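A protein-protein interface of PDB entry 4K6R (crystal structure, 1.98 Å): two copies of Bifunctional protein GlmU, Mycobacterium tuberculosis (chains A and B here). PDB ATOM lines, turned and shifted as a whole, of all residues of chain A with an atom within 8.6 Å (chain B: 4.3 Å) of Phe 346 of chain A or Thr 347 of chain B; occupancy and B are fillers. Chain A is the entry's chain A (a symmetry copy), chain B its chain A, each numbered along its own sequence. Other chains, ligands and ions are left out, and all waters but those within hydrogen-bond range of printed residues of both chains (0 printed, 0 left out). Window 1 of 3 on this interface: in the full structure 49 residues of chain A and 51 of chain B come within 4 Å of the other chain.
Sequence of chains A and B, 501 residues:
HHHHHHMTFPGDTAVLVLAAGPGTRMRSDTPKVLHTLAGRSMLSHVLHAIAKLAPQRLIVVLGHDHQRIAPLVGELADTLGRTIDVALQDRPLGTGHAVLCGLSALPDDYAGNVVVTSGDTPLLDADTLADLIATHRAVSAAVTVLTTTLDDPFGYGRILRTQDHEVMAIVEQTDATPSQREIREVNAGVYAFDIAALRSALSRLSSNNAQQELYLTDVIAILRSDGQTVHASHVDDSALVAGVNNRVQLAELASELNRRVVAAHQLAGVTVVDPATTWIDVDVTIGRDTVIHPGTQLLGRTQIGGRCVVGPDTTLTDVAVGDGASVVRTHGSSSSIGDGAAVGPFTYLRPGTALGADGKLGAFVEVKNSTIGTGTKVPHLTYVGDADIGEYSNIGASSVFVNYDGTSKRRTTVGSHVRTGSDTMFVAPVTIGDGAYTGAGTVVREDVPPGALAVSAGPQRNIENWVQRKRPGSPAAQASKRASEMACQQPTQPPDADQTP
Among the printed residues, merely in contact across the chains: Val 328 of chain A with His 331 of chain B, Pro 345 of chain A with His 331 of chain B, Pro 345 of chain A with Tyr 348 of chain B, Phe 346 of chain A with Arg 329 of chain B, Phe 346 of chain A with Thr 347 of chain B, Ala 363 of chain A with Tyr 348 of chain B, Phe 364 of chain A with Phe 346 of chain B and Phe 364 of chain A with Val 365 of chain B.
Arg 329 of chain A touches His 331 of chain B, but with the chains exchanged His 331 of chain A does not touch Arg 329 of chain B (10.2 Å).
Pro 345 of chain A touches His 331 of chain B, but with the chains exchanged His 331 of chain A does not touch Pro 345 of chain B (14.5 Å).
Pro 345 of chain A touches Tyr 348 of chain B, but with the chains exchanged Tyr 348 of chain A does not touch Pro 345 of chain B (14.2 Å).
O of Phe 346 of chain A sits at hydrogen-bond distance from N of Phe 364 of chain A.
The side-chain hydroxyl (OG1) of Thr 314 of chain A lies within hydrogen-bond range of the backbone NH (N) of Arg 329 of chain A (2.9 Å).
N of Ala 363 of chain A is in hydrogen-bond range of O of Pro 379 of chain A (3.2 Å).
The backbone carbonyl oxygen of Arg 329 of chain B is in hydrogen-bond range of the backbone NH of Thr 347 of chain B (3.3 Å).
OG1 of Thr 347 of chain B is in hydrogen-bond range of O of Gly 362 of chain B, at 2.7 Å.
NE of Arg 329 of chain A lies within hydrogen-bond range of ND1 of His 331 of chain B.
Of the printed residues of chain B, Pro 345 of chain A touches His 331 and Tyr 348.
Of the printed residues of chain B, Phe 346 of chain A touches Arg 329 and Thr 347.
Tyr 348 of chain A touches none of the printed residues of chain B.
Leu 381 of chain A touches none of the printed residues of chain B.
Printed residues of chain A within 4 Å of His 331 of chain B: Val 328, Arg 329 and Pro 345.
No residue of chain A comes within 4 Å of Gly 344 of chain B.
Thr 347 of chain B touches just one residue of chain A: Phe 346.
No residue of chain A comes within 4 Å of Gly 362 of chain B.
The nearest printed residue of chain B that does not touch Phe 346 of chain A is His 331 of chain B (4.01 Å).
The nearest residue of chain A that does not touch Thr 347 of chain B is Phe 364 of chain A (4.3 Å).
The nearest printed residue of chain A that does not touch Tyr 348 of chain B is Phe 364 of chain A (4.2 Å).
Of the 25 printed residues of chain A, 6 touch a printed residue of chain B.
Of the 13 printed residues of chain B, 6 touch a printed residue of chain A.
Printed residues of chain B that touch a printed residue of chain A: Arg 329, His 331, Phe 346, Thr 347, Tyr 348 and Val 365.
Along chain B the printed residues that touch a printed residue of chain A span positions 329 to 365.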
ATOM      1  N   PRO A 312     -25.190  16.771  13.809  1.00  0.00           N
ATOM      2  CA  PRO A 312     -24.729  16.165  12.569  1.00  0.00           C
ATOM      3  C   PRO A 312     -24.398  14.703  12.783  1.00  0.00           C
ATOM      4  O   PRO A 312     -24.379  14.235  13.911  1.00  0.00           O
ATOM      5  CB  PRO A 312     -23.434  16.929  12.281  1.00  0.00           C
ATOM      6  CG  PRO A 312     -22.845  17.168  13.713  1.00  0.00           C
ATOM      7  CD  PRO A 312     -24.163  17.705  14.390  1.00  0.00           C
ATOM      8  N   ASP A 313     -24.050  14.013  11.697  1.00  0.00           N
ATOM      9  CA  ASP A 313     -23.573  12.625  11.792  1.00  0.00           C
ATOM     10  C   ASP A 313     -24.473  11.704  12.586  1.00  0.00           C
ATOM     11  O   ASP A 313     -23.995  10.919  13.419  1.00  0.00           O
ATOM     12  CB  ASP A 313     -22.164  12.630  12.372  1.00  0.00           C
ATOM     13  CG  ASP A 313     -21.171  13.373  11.443  1.00  0.00           C
ATOM     14  OD1 ASP A 313     -21.528  13.874  10.342  1.00  0.00           O
ATOM     15  OD2 ASP A 313     -20.015  13.347  11.733  1.00  0.00           O
ATOM     16  N   THR A 314     -25.758  11.766  12.274  1.00  0.00           N
ATOM     17  CA  THR A 314     -26.734  10.934  12.920  1.00  0.00           C
ATOM     18  C   THR A 314     -27.310   9.982  11.856  1.00  0.00           C
ATOM     19  O   THR A 314     -27.591  10.408  10.694  1.00  0.00           O
ATOM     20  CB  THR A 314     -27.767  11.818  13.568  1.00  0.00           C
ATOM     21  OG1 THR A 314     -27.285  12.305  14.872  1.00  0.00           O
ATOM     22  CG2 THR A 314     -29.120  11.057  13.860  1.00  0.00           C
ATOM     23  N   VAL A 327     -31.024  14.999  18.880  1.00  0.00           N
ATOM     24  CA  VAL A 327     -30.540  13.667  18.593  1.00  0.00           C
ATOM     25  C   VAL A 327     -29.270  13.884  17.721  1.00  0.00           C
ATOM     26  O   VAL A 327     -29.341  14.061  16.464  1.00  0.00           O
ATOM     27  CB  VAL A 327     -31.584  12.821  17.804  1.00  0.00           C
ATOM     28  CG1 VAL A 327     -31.032  11.362  17.641  1.00  0.00           C
ATOM     29  CG2 VAL A 327     -32.908  12.762  18.578  1.00  0.00           C
ATOM     30  N   VAL A 328     -28.129  13.894  18.395  1.00  0.00           N
ATOM     31  CA  VAL A 328     -26.906  14.471  17.803  1.00  0.00           C
ATOM     32  C   VAL A 328     -25.870  13.354  17.781  1.00  0.00           C
ATOM     33  O   VAL A 328     -25.749  12.636  18.767  1.00  0.00           O
ATOM     34  CB  VAL A 328     -26.357  15.570  18.736  1.00  0.00           C
ATOM     35  CG1 VAL A 328     -24.966  16.011  18.268  1.00  0.00           C
ATOM     36  CG2 VAL A 328     -27.363  16.814  18.721  1.00  0.00           C
ATOM     37  N   ARG A 329     -25.136  13.211  16.660  1.00  0.00           N
ATOM     38  CA  ARG A 329     -24.095  12.165  16.513  1.00  0.00           C
ATOM     39  C   ARG A 329     -24.588  10.834  17.104  1.00  0.00           C
ATOM     40  O   ARG A 329     -23.924  10.237  17.951  1.00  0.00           O
ATOM     41  CB  ARG A 329     -22.811  12.591  17.180  1.00  0.00           C
ATOM     42  CG  ARG A 329     -22.105  13.670  16.397  1.00  0.00           C
ATOM     43  CD  ARG A 329     -20.663  13.929  16.943  1.00  0.00           C
ATOM     44  NE  ARG A 329     -20.172  15.045  16.188  1.00  0.00           N
ATOM     45  CZ  ARG A 329     -19.492  14.917  15.070  1.00  0.00           C
ATOM     46  NH1 ARG A 329     -19.192  13.679  14.615  1.00  0.00           N
ATOM     47  NH2 ARG A 329     -19.143  16.017  14.395  1.00  0.00           N
ATOM     48  N   THR A 330     -25.766  10.377  16.655  1.00  0.00           N
ATOM     49  CA  THR A 330     -26.411   9.197  17.223  1.00  0.00           C
ATOM     50  C   THR A 330     -26.594   8.171  16.124  1.00  0.00           C
ATOM     51  O   THR A 330     -26.945   8.530  14.989  1.00  0.00           O
ATOM     52  CB  THR A 330     -27.779   9.609  17.839  1.00  0.00           C
ATOM     53  OG1 THR A 330     -27.527  10.399  19.022  1.00  0.00           O
ATOM     54  CG2 THR A 330     -28.603   8.423  18.302  1.00  0.00           C
ATOM     55  N   HIS A 331     -26.358   6.898  16.456  1.00  0.00           N
ATOM     56  CA  HIS A 331     -26.633   5.779  15.498  1.00  0.00           C
ATOM     57  C   HIS A 331     -27.753   4.980  16.178  1.00  0.00           C
ATOM     58  O   HIS A 331     -27.567   4.478  17.277  1.00  0.00           O
ATOM     59  CB  HIS A 331     -25.375   4.876  15.422  1.00  0.00           C
ATOM     60  CG  HIS A 331     -25.329   4.013  14.213  1.00  0.00           C
ATOM     61  ND1 HIS A 331     -25.046   4.515  12.957  1.00  0.00           N
ATOM     62  CD2 HIS A 331     -25.560   2.683  14.064  1.00  0.00           C
ATOM     63  CE1 HIS A 331     -25.112   3.526  12.081  1.00  0.00           C
ATOM     64  NE2 HIS A 331     -25.424   2.407  12.723  1.00  0.00           N
ATOM     65  N   VAL A 343     -30.362  13.273  23.121  1.00  0.00           N
ATOM     66  CA  VAL A 343     -29.645  12.053  22.884  1.00  0.00           C
ATOM     67  C   VAL A 343     -28.303  12.478  22.202  1.00  0.00           C
ATOM     68  O   VAL A 343     -28.328  13.263  21.288  1.00  0.00           O
ATOM     69  CB  VAL A 343     -30.470  11.134  21.948  1.00  0.00           C
ATOM     70  CG1 VAL A 343     -29.630   9.895  21.616  1.00  0.00           C
ATOM     71  CG2 VAL A 343     -31.842  10.726  22.698  1.00  0.00           C
ATOM     72  N   GLY A 344     -27.152  11.956  22.622  1.00  0.00           N
ATOM     73  CA  GLY A 344     -25.898  12.330  21.930  1.00  0.00           C
ATOM     74  C   GLY A 344     -25.023  13.266  22.751  1.00  0.00           C
ATOM     75  O   GLY A 344     -25.434  13.715  23.820  1.00  0.00           O
ATOM     76  N   PRO A 345     -23.803  13.598  22.265  1.00  0.00           N
ATOM     77  CA  PRO A 345     -23.251  13.078  21.046  1.00  0.00           C
ATOM     78  C   PRO A 345     -22.596  11.682  21.307  1.00  0.00           C
ATOM     79  O   PRO A 345     -22.237  11.341  22.437  1.00  0.00           O
ATOM     80  CB  PRO A 345     -22.180  14.096  20.663  1.00  0.00           C
ATOM     81  CG  PRO A 345     -21.644  14.599  21.972  1.00  0.00           C
ATOM     82  CD  PRO A 345     -22.877  14.522  22.976  1.00  0.00           C
ATOM     83  N   PHE A 346     -22.457  10.875  20.247  1.00  0.00           N
ATOM     84  CA  PHE A 346     -21.827   9.554  20.361  1.00  0.00           C
ATOM     85  C   PHE A 346     -22.670   8.572  21.144  1.00  0.00           C
ATOM     86  O   PHE A 346     -22.206   8.025  22.167  1.00  0.00           O
ATOM     87  CB  PHE A 346     -20.405   9.602  20.949  1.00  0.00           C
ATOM     88  CG  PHE A 346     -19.487  10.624  20.262  1.00  0.00           C
ATOM     89  CD1 PHE A 346     -19.045  10.455  18.953  1.00  0.00           C
ATOM     90  CD2 PHE A 346     -19.091  11.772  20.968  1.00  0.00           C
ATOM     91  CE1 PHE A 346     -18.173  11.466  18.311  1.00  0.00           C
ATOM     92  CE2 PHE A 346     -18.213  12.703  20.380  1.00  0.00           C
ATOM     93  CZ  PHE A 346     -17.751  12.574  19.073  1.00  0.00           C
ATOM     94  N   THR A 347     -23.873   8.287  20.611  1.00  0.00           N
ATOM     95  CA  THR A 347     -24.837   7.421  21.399  1.00  0.00           C
ATOM     96  C   THR A 347     -25.355   6.371  20.453  1.00  0.00           C
ATOM     97  O   THR A 347     -25.641   6.715  19.317  1.00  0.00           O
ATOM     98  CB  THR A 347     -26.024   8.269  21.919  1.00  0.00           C
ATOM     99  OG1 THR A 347     -25.492   9.351  22.738  1.00  0.00           O
ATOM    100  CG2 THR A 347     -26.997   7.435  22.799  1.00  0.00           C
ATOM    101  N   TYR A 348     -25.530   5.121  20.948  1.00  0.00           N
ATOM    102  CA  TYR A 348     -25.894   3.964  20.090  1.00  0.00           C
ATOM    103  C   TYR A 348     -27.227   3.409  20.648  1.00  0.00           C
ATOM    104  O   TYR A 348     -27.279   3.007  21.836  1.00  0.00           O
ATOM    105  CB  TYR A 348     -24.804   2.865  20.193  1.00  0.00           C
ATOM    106  CG  TYR A 348     -25.013   1.639  19.346  1.00  0.00           C
ATOM    107  CD1 TYR A 348     -25.875   1.648  18.234  1.00  0.00           C
ATOM    108  CD2 TYR A 348     -24.337   0.478  19.640  1.00  0.00           C
ATOM    109  CE1 TYR A 348     -26.029   0.493  17.447  1.00  0.00           C
ATOM    110  CE2 TYR A 348     -24.561  -0.696  18.894  1.00  0.00           C
ATOM    111  CZ  TYR A 348     -25.388  -0.660  17.836  1.00  0.00           C
ATOM    112  OH  TYR A 348     -25.546  -1.773  17.110  1.00  0.00           O
ATOM    113  N   LEU A 349     -28.289   3.536  19.853  1.00  0.00           N
ATOM    114  CA  LEU A 349     -29.607   3.001  20.292  1.00  0.00           C
ATOM    115  C   LEU A 349     -29.912   1.738  19.472  1.00  0.00           C
ATOM    116  O   LEU A 349     -29.943   1.807  18.229  1.00  0.00           O
ATOM    117  CB  LEU A 349     -30.744   4.008  20.083  1.00  0.00           C
ATOM    118  CG  LEU A 349     -30.483   5.439  20.696  1.00  0.00           C
ATOM    119  CD1 LEU A 349     -31.740   6.277  20.565  1.00  0.00           C
ATOM    120  CD2 LEU A 349     -30.155   5.350  22.192  1.00  0.00           C
ATOM    121  N   LEU A 361     -29.834  10.569  27.025  1.00  0.00           N
ATOM    122  CA  LEU A 361     -28.825   9.500  26.834  1.00  0.00           C
ATOM    123  C   LEU A 361     -27.588  10.197  26.261  1.00  0.00           C
ATOM    124  O   LEU A 361     -27.643  10.709  25.156  1.00  0.00           O
ATOM    125  CB  LEU A 361     -29.352   8.391  25.887  1.00  0.00           C
ATOM    126  CG  LEU A 361     -30.634   7.649  26.421  1.00  0.00           C
ATOM    127  CD1 LEU A 361     -31.200   6.705  25.300  1.00  0.00           C
ATOM    128  CD2 LEU A 361     -30.360   6.899  27.697  1.00  0.00           C
ATOM    129  N   GLY A 362     -26.512  10.271  27.057  1.00  0.00           N
ATOM    130  CA  GLY A 362     -25.348  11.047  26.706  1.00  0.00           C
ATOM    131  C   GLY A 362     -24.224  10.339  25.967  1.00  0.00           C
ATOM    132  O   GLY A 362     -24.442   9.310  25.263  1.00  0.00           O
ATOM    133  N   ALA A 363     -23.030  10.934  26.041  1.00  0.00           N
ATOM    134  CA  ALA A 363     -21.900  10.452  25.236  1.00  0.00           C
ATOM    135  C   ALA A 363     -21.371   9.117  25.692  1.00  0.00           C
ATOM    136  O   ALA A 363     -21.164   8.880  26.914  1.00  0.00           O
ATOM    137  CB  ALA A 363     -20.751  11.525  25.205  1.00  0.00           C
ATOM    138  N   PHE A 364     -21.138   8.214  24.700  1.00  0.00           N
ATOM    139  CA  PHE A 364     -20.539   6.890  24.922  1.00  0.00           C
ATOM    140  C   PHE A 364     -21.531   6.062  25.752  1.00  0.00           C
ATOM    141  O   PHE A 364     -21.173   5.337  26.680  1.00  0.00           O
ATOM    142  CB  PHE A 364     -19.120   6.972  25.523  1.00  0.00           C
ATOM    143  CG  PHE A 364     -18.308   8.159  24.961  1.00  0.00           C
ATOM    144  CD1 PHE A 364     -18.167   8.341  23.571  1.00  0.00           C
ATOM    145  CD2 PHE A 364     -17.824   9.120  25.809  1.00  0.00           C
ATOM    146  CE1 PHE A 364     -17.495   9.437  23.052  1.00  0.00           C
ATOM    147  CE2 PHE A 364     -17.130  10.234  25.308  1.00  0.00           C
ATOM    148  CZ  PHE A 364     -16.960  10.412  23.951  1.00  0.00           C
ATOM    149  N   VAL A 365     -22.798   6.227  25.395  1.00  0.00           N
ATOM    150  CA  VAL A 365     -23.882   5.420  26.040  1.00  0.00           C
ATOM    151  C   VAL A 365     -24.477   4.483  24.975  1.00  0.00           C
ATOM    152  O   VAL A 365     -24.731   4.925  23.842  1.00  0.00           O
ATOM    153  CB  VAL A 365     -24.950   6.395  26.633  1.00  0.00           C
ATOM    154  CG1 VAL A 365     -26.231   5.647  27.111  1.00  0.00           C
ATOM    155  CG2 VAL A 365     -24.319   7.103  27.854  1.00  0.00           C
ATOM    156  N   GLU A 366     -24.730   3.218  25.331  1.00  0.00           N
ATOM    157  CA  GLU A 366     -25.465   2.361  24.398  1.00  0.00           C
ATOM    158  C   GLU A 366     -26.666   1.805  25.159  1.00  0.00           C
ATOM    159  O   GLU A 366     -26.515   1.432  26.326  1.00  0.00           O
ATOM    160  CB  GLU A 366     -24.575   1.149  23.996  1.00  0.00           C
ATOM    161  CG  GLU A 366     -25.405   0.049  23.270  1.00  0.00           C
ATOM    162  CD  GLU A 366     -24.510  -1.087  22.763  1.00  0.00           C
ATOM    163  OE1 GLU A 366     -23.283  -0.848  22.540  1.00  0.00           O
ATOM    164  OE2 GLU A 366     -25.033  -2.198  22.581  1.00  0.00           O
ATOM    165  N   PRO A 379     -26.117   9.810  31.458  1.00  0.00           N
ATOM    166  CA  PRO A 379     -25.336  10.736  30.634  1.00  0.00           C
ATOM    167  C   PRO A 379     -23.949  10.281  30.162  1.00  0.00           C
ATOM    168  O   PRO A 379     -23.419  10.924  29.263  1.00  0.00           O
ATOM    169  CB  PRO A 379     -25.108  11.923  31.580  1.00  0.00           C
ATOM    170  CG  PRO A 379     -25.183  11.337  32.966  1.00  0.00           C
ATOM    171  CD  PRO A 379     -26.268  10.281  32.842  1.00  0.00           C
ATOM    172  N   HIS A 380     -23.305   9.322  30.792  1.00  0.00           N
ATOM    173  CA  HIS A 380     -21.915   9.013  30.443  1.00  0.00           C
ATOM    174  C   HIS A 380     -21.491   7.540  30.427  1.00  0.00           C
ATOM    175  O   HIS A 380     -21.604   6.893  31.407  1.00  0.00           O
ATOM    176  CB  HIS A 380     -20.966   9.663  31.442  1.00  0.00           C
ATOM    177  CG  HIS A 380     -21.201  11.106  31.712  1.00  0.00           C
ATOM    178  ND1 HIS A 380     -20.909  12.082  30.804  1.00  0.00           N
ATOM    179  CD2 HIS A 380     -21.613  11.746  32.821  1.00  0.00           C
ATOM    180  CE1 HIS A 380     -21.153  13.261  31.329  1.00  0.00           C
ATOM    181  NE2 HIS A 380     -21.593  13.081  32.548  1.00  0.00           N
ATOM    182  N   LEU A 381     -20.918   7.078  29.339  1.00  0.00           N
ATOM    183  CA  LEU A 381     -20.080   5.895  29.349  1.00  0.00           C
ATOM    184  C   LEU A 381     -20.732   4.636  29.936  1.00  0.00           C
ATOM    185  O   LEU A 381     -20.165   3.968  30.719  1.00  0.00           O
ATOM    186  CB  LEU A 381     -18.757   6.207  30.053  1.00  0.00           C
ATOM    187  CG  LEU A 381     -17.754   7.136  29.365  1.00  0.00           C
ATOM    188  CD1 LEU A 381     -16.871   7.926  30.302  1.00  0.00           C
ATOM    189  CD2 LEU A 381     -16.977   6.439  28.332  1.00  0.00           C
ATOM    190  N   THR A 382     -21.960   4.388  29.545  1.00  0.00           N
ATOM    191  CA  THR A 382     -22.796   3.376  30.145  1.00  0.00           C
ATOM    192  C   THR A 382     -23.524   2.476  29.123  1.00  0.00           C
ATOM    193  O   THR A 382     -23.924   2.921  28.115  1.00  0.00           O
ATOM    194  CB  THR A 382     -23.799   4.077  31.096  1.00  0.00           C
ATOM    195  OG1 THR A 382     -23.114   4.629  32.198  1.00  0.00           O
ATOM    196  CG2 THR A 382     -24.907   3.185  31.563  1.00  0.00           C
ATOM    197  N   ARG B 329     -12.471  13.611  14.754  1.00  0.00           N
ATOM    198  CA  ARG B 329     -13.765  13.040  15.197  1.00  0.00           C
ATOM    199  C   ARG B 329     -14.141  13.584  16.586  1.00  0.00           C
ATOM    200  O   ARG B 329     -14.406  12.818  17.511  1.00  0.00           O
ATOM    201  CB  ARG B 329     -13.705  11.533  15.224  1.00  0.00           C
ATOM    202  CG  ARG B 329     -13.708  10.949  13.832  1.00  0.00           C
ATOM    203  CD  ARG B 329     -13.904   9.399  13.859  1.00  0.00           C
ATOM    204  NE  ARG B 329     -13.766   8.981  12.494  1.00  0.00           N
ATOM    205  CZ  ARG B 329     -14.782   8.877  11.665  1.00  0.00           C
ATOM    206  NH1 ARG B 329     -16.033   9.130  12.115  1.00  0.00           N
ATOM    207  NH2 ARG B 329     -14.547   8.555  10.389  1.00  0.00           N
ATOM    208  N   THR B 330     -14.154  14.917  16.725  1.00  0.00           N
ATOM    209  CA  THR B 330     -14.367  15.563  18.017  1.00  0.00           C
ATOM    210  C   THR B 330     -15.594  16.445  17.921  1.00  0.00           C
ATOM    211  O   THR B 330     -15.799  17.118  16.899  1.00  0.00           O
ATOM    212  CB  THR B 330     -13.105  16.396  18.385  1.00  0.00           C
ATOM    213  OG1 THR B 330     -12.028  15.484  18.691  1.00  0.00           O
ATOM    214  CG2 THR B 330     -13.295  17.243  19.629  1.00  0.00           C
ATOM    215  N   HIS B 331     -16.411  16.442  18.979  1.00  0.00           N
ATOM    216  CA  HIS B 331     -17.584  17.370  19.061  1.00  0.00           C
ATOM    217  C   HIS B 331     -17.248  18.283  20.247  1.00  0.00           C
ATOM    218  O   HIS B 331     -17.087  17.806  21.361  1.00  0.00           O
ATOM    219  CB  HIS B 331     -18.842  16.543  19.431  1.00  0.00           C
ATOM    220  CG  HIS B 331     -20.123  17.226  19.113  1.00  0.00           C
ATOM    221  ND1 HIS B 331     -20.589  17.358  17.820  1.00  0.00           N
ATOM    222  CD2 HIS B 331     -21.023  17.843  19.922  1.00  0.00           C
ATOM    223  CE1 HIS B 331     -21.724  18.036  17.845  1.00  0.00           C
ATOM    224  NE2 HIS B 331     -22.009  18.344  19.105  1.00  0.00           N
ATOM    225  N   VAL B 343      -6.470  15.523  20.175  1.00  0.00           N
ATOM    226  CA  VAL B 343      -7.784  15.318  20.714  1.00  0.00           C
ATOM    227  C   VAL B 343      -8.486  14.311  19.745  1.00  0.00           C
ATOM    228  O   VAL B 343      -8.424  14.496  18.555  1.00  0.00           O
ATOM    229  CB  VAL B 343      -8.549  16.665  20.756  1.00  0.00           C
ATOM    230  CG1 VAL B 343      -9.985  16.396  21.220  1.00  0.00           C
ATOM    231  CG2 VAL B 343      -7.785  17.665  21.768  1.00  0.00           C
ATOM    232  N   GLY B 344      -9.158  13.273  20.239  1.00  0.00           N
ATOM    233  CA  GLY B 344      -9.859  12.360  19.308  1.00  0.00           C
ATOM    234  C   GLY B 344      -9.168  11.013  19.165  1.00  0.00           C
ATOM    235  O   GLY B 344      -8.082  10.816  19.707  1.00  0.00           O
ATOM    236  N   PRO B 345      -9.771  10.058  18.417  1.00  0.00           N
ATOM    237  CA  PRO B 345     -11.055  10.210  17.794  1.00  0.00           C
ATOM    238  C   PRO B 345     -12.191   9.904  18.823  1.00  0.00           C
ATOM    239  O   PRO B 345     -11.981   9.220  19.828  1.00  0.00           O
ATOM    240  CB  PRO B 345     -11.055   9.161  16.686  1.00  0.00           C
ATOM    241  CG  PRO B 345     -10.240   8.024  17.235  1.00  0.00           C
ATOM    242  CD  PRO B 345      -9.172   8.712  18.194  1.00  0.00           C
ATOM    243  N   PHE B 346     -13.396  10.430  18.564  1.00  0.00           N
ATOM    244  CA  PHE B 346     -14.548  10.185  19.440  1.00  0.00           C
ATOM    245  C   PHE B 346     -14.414  10.863  20.785  1.00  0.00           C
ATOM    246  O   PHE B 346     -14.454  10.185  21.834  1.00  0.00           O
ATOM    247  CB  PHE B 346     -14.859   8.690  19.640  1.00  0.00           C
ATOM    248  CG  PHE B 346     -14.949   7.897  18.329  1.00  0.00           C
ATOM    249  CD1 PHE B 346     -15.986   8.090  17.420  1.00  0.00           C
ATOM    250  CD2 PHE B 346     -13.949   6.957  18.026  1.00  0.00           C
ATOM    251  CE1 PHE B 346     -16.038   7.320  16.154  1.00  0.00           C
ATOM    252  CE2 PHE B 346     -14.031   6.182  16.852  1.00  0.00           C
ATOM    253  CZ  PHE B 346     -15.048   6.346  15.916  1.00  0.00           C
ATOM    254  N   THR B 347     -14.340  12.207  20.753  1.00  0.00           N
ATOM    255  CA  THR B 347     -14.065  12.957  22.041  1.00  0.00           C
ATOM    256  C   THR B 347     -15.070  14.075  22.119  1.00  0.00           C
ATOM    257  O   THR B 347     -15.315  14.697  21.097  1.00  0.00           O
ATOM    258  CB  THR B 347     -12.636  13.555  22.022  1.00  0.00           C
ATOM    259  OG1 THR B 347     -11.685  12.470  21.828  1.00  0.00           O
ATOM    260  CG2 THR B 347     -12.284  14.269  23.358  1.00  0.00           C
ATOM    261  N   TYR B 348     -15.589  14.358  23.338  1.00  0.00           N
ATOM    262  CA  TYR B 348     -16.694  15.334  23.531  1.00  0.00           C
ATOM    263  C   TYR B 348     -16.153  16.418  24.496  1.00  0.00           C
ATOM    264  O   TYR B 348     -15.763  16.086  25.641  1.00  0.00           O
ATOM    265  CB  TYR B 348     -17.912  14.633  24.187  1.00  0.00           C
ATOM    266  CG  TYR B 348     -19.130  15.486  24.411  1.00  0.00           C
ATOM    267  CD1 TYR B 348     -19.327  16.691  23.711  1.00  0.00           C
ATOM    268  CD2 TYR B 348     -20.094  15.086  25.306  1.00  0.00           C
ATOM    269  CE1 TYR B 348     -20.488  17.454  23.925  1.00  0.00           C
ATOM    270  CE2 TYR B 348     -21.213  15.898  25.573  1.00  0.00           C
ATOM    271  CZ  TYR B 348     -21.379  17.043  24.888  1.00  0.00           C
ATOM    272  OH  TYR B 348     -22.476  17.774  25.120  1.00  0.00           O
ATOM    273  N   LEU B 349     -16.003  17.637  23.977  1.00  0.00           N
ATOM    274  CA  LEU B 349     -15.522  18.750  24.839  1.00  0.00           C
ATOM    275  C   LEU B 349     -16.706  19.688  25.122  1.00  0.00           C
ATOM    276  O   LEU B 349     -17.320  20.204  24.169  1.00  0.00           O
ATOM    277  CB  LEU B 349     -14.403  19.561  24.173  1.00  0.00           C
ATOM    278  CG  LEU B 349     -13.194  18.702  23.633  1.00  0.00           C
ATOM    279  CD1 LEU B 349     -12.095  19.630  23.154  1.00  0.00           C
ATOM    280  CD2 LEU B 349     -12.594  17.830  24.743  1.00  0.00           C
ATOM    281  N   LEU B 361      -6.476  14.188  24.764  1.00  0.00           N
ATOM    282  CA  LEU B 361      -7.795  13.670  25.196  1.00  0.00           C
ATOM    283  C   LEU B 361      -8.199  12.637  24.138  1.00  0.00           C
ATOM    284  O   LEU B 361      -8.418  13.000  22.995  1.00  0.00           O
ATOM    285  CB  LEU B 361      -8.838  14.810  25.314  1.00  0.00           C
ATOM    286  CG  LEU B 361      -8.466  15.910  26.378  1.00  0.00           C
ATOM    287  CD1 LEU B 361      -9.469  17.113  26.264  1.00  0.00           C
ATOM    288  CD2 LEU B 361      -8.421  15.351  27.774  1.00  0.00           C
ATOM    289  N   GLY B 362      -8.217  11.353  24.523  1.00  0.00           N
ATOM    290  CA  GLY B 362      -8.410  10.274  23.586  1.00  0.00           C
ATOM    291  C   GLY B 362      -9.829   9.782  23.359  1.00  0.00           C
ATOM    292  O   GLY B 362     -10.829  10.533  23.559  1.00  0.00           O
ATOM    293  N   VAL B 365     -13.672   9.864  25.480  1.00  0.00           N
ATOM    294  CA  VAL B 365     -13.378  10.762  26.641  1.00  0.00           C
ATOM    295  C   VAL B 365     -14.333  11.965  26.567  1.00  0.00           C
ATOM    296  O   VAL B 365     -14.524  12.531  25.479  1.00  0.00           O
ATOM    297  CB  VAL B 365     -11.878  11.193  26.576  1.00  0.00           C
ATOM    298  CG1 VAL B 365     -11.540  12.315  27.603  1.00  0.00           C
ATOM    299  CG2 VAL B 365     -11.013   9.956  26.911  1.00  0.00           C
